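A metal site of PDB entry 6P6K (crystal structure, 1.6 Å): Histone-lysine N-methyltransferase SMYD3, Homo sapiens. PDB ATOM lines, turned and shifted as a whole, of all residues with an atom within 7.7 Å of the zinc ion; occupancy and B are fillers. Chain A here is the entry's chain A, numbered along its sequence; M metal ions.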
ATOM      1  N   ARG A  65      23.318 -12.018 -26.163  1.00  0.00           N
ATOM      2  CA  ARG A  65      22.616 -13.281 -26.366  1.00  0.00           C
ATOM      3  C   ARG A  65      23.577 -14.383 -26.766  1.00  0.00           C
ATOM      4  O   ARG A  65      24.540 -14.158 -27.507  1.00  0.00           O
ATOM      5  CB  ARG A  65      21.540 -13.122 -27.452  1.00  0.00           C
ATOM      6  N   CYS A  66      23.323 -15.595 -26.259  1.00  0.00           N
ATOM      7  CA  CYS A  66      24.004 -16.779 -26.773  1.00  0.00           C
ATOM      8  C   CYS A  66      23.670 -16.955 -28.245  1.00  0.00           C
ATOM      9  O   CYS A  66      22.499 -17.092 -28.607  1.00  0.00           O
ATOM     10  CB  CYS A  66      23.582 -18.008 -25.969  1.00  0.00           C
ATOM     11  SG  CYS A  66      24.148 -19.598 -26.633  1.00  0.00           S
ATOM     12  N   SER A  67      24.675 -16.961 -29.105  1.00  0.00           N
ATOM     13  CA  SER A  67      24.340 -17.016 -30.530  1.00  0.00           C
ATOM     14  C   SER A  67      23.912 -18.410 -30.966  1.00  0.00           C
ATOM     15  O   SER A  67      23.321 -18.547 -32.036  1.00  0.00           O
ATOM     16  CB  SER A  67      25.507 -16.520 -31.392  1.00  0.00           C
ATOM     17  OG  SER A  67      26.581 -17.448 -31.378  1.00  0.00           O
ATOM     18  N   GLN A  68      24.183 -19.446 -30.160  1.00  0.00           N
ATOM     19  CA  GLN A  68      23.722 -20.775 -30.532  1.00  0.00           C
ATOM     20  C   GLN A  68      22.214 -20.906 -30.342  1.00  0.00           C
ATOM     21  O   GLN A  68      21.512 -21.369 -31.241  1.00  0.00           O
ATOM     22  CB  GLN A  68      24.474 -21.843 -29.735  1.00  0.00           C
ATOM     23  N   CYS A  69      21.701 -20.484 -29.189  1.00  0.00           N
ATOM     24  CA  CYS A  69      20.276 -20.611 -28.886  1.00  0.00           C
ATOM     25  C   CYS A  69      19.487 -19.313 -28.940  1.00  0.00           C
ATOM     26  O   CYS A  69      18.281 -19.367 -29.162  1.00  0.00           O
ATOM     27  CB  CYS A  69      20.083 -21.242 -27.505  1.00  0.00           C
ATOM     28  SG  CYS A  69      20.489 -20.132 -26.149  1.00  0.00           S
ATOM     29  N   ARG A  70      20.134 -18.162 -28.721  1.00  0.00           N
ATOM     30  CA  ARG A  70      19.498 -16.842 -28.728  1.00  0.00           C
ATOM     31  C   ARG A  70      18.472 -16.662 -27.609  1.00  0.00           C
ATOM     32  O   ARG A  70      17.702 -15.690 -27.632  1.00  0.00           O
ATOM     33  CB  ARG A  70      18.850 -16.528 -30.082  1.00  0.00           C
ATOM     34  N   VAL A  71      18.461 -17.545 -26.616  1.00  0.00           N
ATOM     35  CA  VAL A  71      17.552 -17.431 -25.481  1.00  0.00           C
ATOM     36  C   VAL A  71      18.292 -16.948 -24.237  1.00  0.00           C
ATOM     37  O   VAL A  71      17.869 -15.988 -23.596  1.00  0.00           O
ATOM     38  CB  VAL A  71      16.852 -18.780 -25.227  1.00  0.00           C
ATOM     39  CG1 VAL A  71      15.928 -18.685 -24.022  1.00  0.00           C
ATOM     40  CG2 VAL A  71      16.092 -19.224 -26.466  1.00  0.00           C
ATOM     41  N   ALA A  72      19.383 -17.612 -23.880  1.00  0.00           N
ATOM     42  CA  ALA A  72      20.169 -17.194 -22.728  1.00  0.00           C
ATOM     43  C   ALA A  72      20.845 -15.860 -23.026  1.00  0.00           C
ATOM     44  O   ALA A  72      21.456 -15.676 -24.085  1.00  0.00           O
ATOM     45  CB  ALA A  72      21.208 -18.258 -22.384  1.00  0.00           C
ATOM     46  N   LYS A  73      20.733 -14.916 -22.085  1.00  0.00           N
ATOM     47  CA  LYS A  73      21.364 -13.616 -22.229  1.00  0.00           C
ATOM     48  C   LYS A  73      22.210 -13.318 -21.011  1.00  0.00           C
ATOM     49  O   LYS A  73      21.900 -13.750 -19.893  1.00  0.00           O
ATOM     50  CB  LYS A  73      20.315 -12.508 -22.445  1.00  0.00           C
ATOM     51  CG  LYS A  73      19.441 -12.764 -23.663  1.00  0.00           C
ATOM     52  CD  LYS A  73      18.634 -11.537 -24.054  1.00  0.00           C
ATOM     53  CE  LYS A  73      17.676 -11.862 -25.202  1.00  0.00           C
ATOM     54  NZ  LYS A  73      16.694 -10.775 -25.433  1.00  0.00           N
ATOM     55  N   TYR A  74      23.301 -12.572 -21.211  1.00  0.00           N
ATOM     56  CA  TYR A  74      24.313 -12.418 -20.176  1.00  0.00           C
ATOM     57  C   TYR A  74      24.779 -10.978 -20.060  1.00  0.00           C
ATOM     58  O   TYR A  74      24.764 -10.218 -21.036  1.00  0.00           O
ATOM     59  CB  TYR A  74      25.510 -13.324 -20.457  1.00  0.00           C
ATOM     60  CG  TYR A  74      25.135 -14.784 -20.588  1.00  0.00           C
ATOM     61  CD1 TYR A  74      24.958 -15.577 -19.467  1.00  0.00           C
ATOM     62  CD2 TYR A  74      24.952 -15.368 -21.842  1.00  0.00           C
ATOM     63  CE1 TYR A  74      24.615 -16.922 -19.582  1.00  0.00           C
ATOM     64  CE2 TYR A  74      24.617 -16.703 -21.964  1.00  0.00           C
ATOM     65  CZ  TYR A  74      24.445 -17.469 -20.829  1.00  0.00           C
ATOM     66  OH  TYR A  74      24.113 -18.795 -20.949  1.00  0.00           O
ATOM     67  N   GLN A  80      28.724 -15.207 -19.517  1.00  0.00           N
ATOM     68  CA  GLN A  80      28.383 -16.135 -20.589  1.00  0.00           C
ATOM     69  C   GLN A  80      29.313 -17.345 -20.581  1.00  0.00           C
ATOM     70  O   GLN A  80      28.854 -18.484 -20.706  1.00  0.00           O
ATOM     71  CB  GLN A  80      28.432 -15.444 -21.954  1.00  0.00           C
ATOM     72  CG  GLN A  80      28.109 -16.398 -23.095  1.00  0.00           C
ATOM     73  CD  GLN A  80      27.856 -15.723 -24.429  1.00  0.00           C
ATOM     74  OE1 GLN A  80      27.798 -14.499 -24.515  1.00  0.00           O
ATOM     75  NE2 GLN A  80      27.698 -16.528 -25.472  1.00  0.00           N
ATOM     76  N   TRP A  84      28.524 -21.434 -19.358  1.00  0.00           N
ATOM     77  CA  TRP A  84      28.478 -22.374 -20.476  1.00  0.00           C
ATOM     78  C   TRP A  84      28.354 -23.827 -20.029  1.00  0.00           C
ATOM     79  O   TRP A  84      27.520 -24.542 -20.599  1.00  0.00           O
ATOM     80  CB  TRP A  84      29.691 -22.183 -21.403  1.00  0.00           C
ATOM     81  CG  TRP A  84      29.729 -23.224 -22.489  1.00  0.00           C
ATOM     82  CD1 TRP A  84      30.657 -24.197 -22.648  1.00  0.00           C
ATOM     83  CD2 TRP A  84      28.765 -23.414 -23.537  1.00  0.00           C
ATOM     84  NE1 TRP A  84      30.348 -24.970 -23.745  1.00  0.00           N
ATOM     85  CE2 TRP A  84      29.190 -24.514 -24.301  1.00  0.00           C
ATOM     86  CE3 TRP A  84      27.587 -22.748 -23.910  1.00  0.00           C
ATOM     87  CZ2 TRP A  84      28.481 -24.967 -25.421  1.00  0.00           C
ATOM     88  CZ3 TRP A  84      26.882 -23.196 -25.006  1.00  0.00           C
ATOM     89  CH2 TRP A  84      27.332 -24.298 -25.748  1.00  0.00           C
ATOM     90  N   HIS A  87      24.889 -24.535 -19.214  1.00  0.00           N
ATOM     91  CA  HIS A  87      23.995 -24.141 -20.291  1.00  0.00           C
ATOM     92  C   HIS A  87      24.154 -25.002 -21.535  1.00  0.00           C
ATOM     93  O   HIS A  87      23.235 -25.021 -22.373  1.00  0.00           O
ATOM     94  CB  HIS A  87      24.240 -22.669 -20.673  1.00  0.00           C
ATOM     95  CG  HIS A  87      23.433 -22.201 -21.851  1.00  0.00           C
ATOM     96  ND1 HIS A  87      22.060 -22.101 -21.824  1.00  0.00           N
ATOM     97  CD2 HIS A  87      23.812 -21.813 -23.093  1.00  0.00           C
ATOM     98  CE1 HIS A  87      21.629 -21.673 -22.992  1.00  0.00           C
ATOM     99  NE2 HIS A  87      22.668 -21.487 -23.789  1.00  0.00           N
ATOM    100  N   LYS A  88      25.286 -25.706 -21.674  1.00  0.00           N
ATOM    101  CA  LYS A  88      25.603 -26.432 -22.901  1.00  0.00           C
ATOM    102  C   LYS A  88      24.461 -27.325 -23.371  1.00  0.00           C
ATOM    103  O   LYS A  88      24.058 -27.285 -24.539  1.00  0.00           O
ATOM    104  CB  LYS A  88      26.874 -27.253 -22.688  1.00  0.00           C
ATOM    105  CG  LYS A  88      27.304 -28.054 -23.901  1.00  0.00           C
ATOM    106  N   GLU A  90      21.156 -27.565 -22.255  1.00  0.00           N
ATOM    107  CA  GLU A  90      19.880 -26.888 -22.496  1.00  0.00           C
ATOM    108  C   GLU A  90      19.930 -26.007 -23.723  1.00  0.00           C
ATOM    109  O   GLU A  90      18.891 -25.744 -24.343  1.00  0.00           O
ATOM    110  CB  GLU A  90      19.450 -26.078 -21.272  1.00  0.00           C
ATOM    111  CG  GLU A  90      20.318 -24.877 -20.999  1.00  0.00           C
ATOM    112  CD  GLU A  90      19.666 -23.849 -20.106  1.00  0.00           C
ATOM    113  OE1 GLU A  90      18.600 -24.128 -19.510  1.00  0.00           O
ATOM    114  OE2 GLU A  90      20.225 -22.742 -20.003  1.00  0.00           O
ATOM    115  N   CYS A  91      21.130 -25.545 -24.114  1.00  0.00           N
ATOM    116  CA  CYS A  91      21.258 -24.712 -25.299  1.00  0.00           C
ATOM    117  C   CYS A  91      20.714 -25.429 -26.529  1.00  0.00           C
ATOM    118  O   CYS A  91      19.934 -24.853 -27.299  1.00  0.00           O
ATOM    119  CB  CYS A  91      22.715 -24.316 -25.481  1.00  0.00           C
ATOM    120  SG  CYS A  91      23.003 -23.201 -26.860  1.00  0.00           S
ATOM    121  N   LYS A  92      21.101 -26.686 -26.726  1.00  0.00           N
ATOM    122  CA  LYS A  92      20.611 -27.461 -27.869  1.00  0.00           C
ATOM    123  C   LYS A  92      19.099 -27.651 -27.814  1.00  0.00           C
ATOM    124  O   LYS A  92      18.441 -27.726 -28.856  1.00  0.00           O
ATOM    125  CB  LYS A  92      21.318 -28.816 -27.930  1.00  0.00           C
ATOM    126  CG  LYS A  92      22.830 -28.730 -28.065  1.00  0.00           C
ATOM    127  N   LEU A  94      16.849 -25.474 -26.185  1.00  0.00           N
ATOM    128  CA  LEU A  94      16.210 -24.192 -26.446  1.00  0.00           C
ATOM    129  C   LEU A  94      16.250 -23.843 -27.924  1.00  0.00           C
ATOM    130  O   LEU A  94      15.310 -23.243 -28.458  1.00  0.00           O
ATOM    131  CB  LEU A  94      16.880 -23.098 -25.619  1.00  0.00           C
ATOM    132  CG  LEU A  94      16.717 -23.206 -24.100  1.00  0.00           C
ATOM    133  CD1 LEU A  94      17.768 -22.372 -23.366  1.00  0.00           C
ATOM    134  CD2 LEU A  94      15.313 -22.787 -23.695  1.00  0.00           C
ATOM    135  N   LYS A  95      17.333 -24.223 -28.610  1.00  0.00           N
ATOM    136  CA  LYS A  95      17.425 -23.954 -30.046  1.00  0.00           C
ATOM    137  C   LYS A  95      16.433 -24.801 -30.821  1.00  0.00           C
ATOM    138  O   LYS A  95      15.748 -24.299 -31.726  1.00  0.00           O
ATOM    139  CB  LYS A  95      18.848 -24.210 -30.546  1.00  0.00           C
ATOM    140  CG  LYS A  95      19.061 -23.829 -32.013  1.00  0.00           C
ATOM    141  CD  LYS A  95      20.454 -24.217 -32.498  1.00  0.00           C
ATOM    142  N   ARG A 107      12.353 -25.642 -17.521  1.00  0.00           N
ATOM    143  CA  ARG A 107      13.748 -25.292 -17.688  1.00  0.00           C
ATOM    144  C   ARG A 107      14.537 -25.577 -16.414  1.00  0.00           C
ATOM    145  O   ARG A 107      15.695 -26.005 -16.468  1.00  0.00           O
ATOM    146  CB  ARG A 107      13.889 -23.833 -18.084  1.00  0.00           C
ATOM    147  CG  ARG A 107      15.316 -23.446 -18.400  1.00  0.00           C
ATOM    148  CD  ARG A 107      15.416 -22.054 -18.936  1.00  0.00           C
ATOM    149  NE  ARG A 107      16.790 -21.730 -19.331  1.00  0.00           N
ATOM    150  CZ  ARG A 107      17.197 -20.503 -19.629  1.00  0.00           C
ATOM    151  NH1 ARG A 107      16.334 -19.494 -19.559  1.00  0.00           N
ATOM    152  NH2 ARG A 107      18.453 -20.274 -19.980  1.00  0.00           N
HETATM  153 ZN    ZN M   1      22.648 -21.124 -25.860  1.00  0.00          ZN
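The side-chain sulfur (SG) of Cys 66 lies close to the backbone NH (N) of Gln 68. The side-chain carboxylate (OE2) of Glu 90 sits at hydrogen-bond distance from a ring nitrogen (ND1) of His 87, at 2.7 Å. The backbone NH (N) of Cys 66 is in hydrogen-bond range of the backbone carbonyl oxygen (O) of Ala 72. The side-chain sulfur of Cys 69 sits close to the backbone NH of Val 71 (3.3 Å). The side-chain sulfur of Cys 69 sits close to the backbone NH of Ala 72 (3.6 Å).
NE2 of His 87 is bound to the zinc ion, 2.1 Å away. SG of Cys 66 binds the zinc ion, at 2.3 Å. SG of Cys 91 binds the zinc ion (2.3 Å). The zinc ion is bound by SG of Cys 69 (2.4 Å). The zinc ion has four donor atoms within binding distance.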
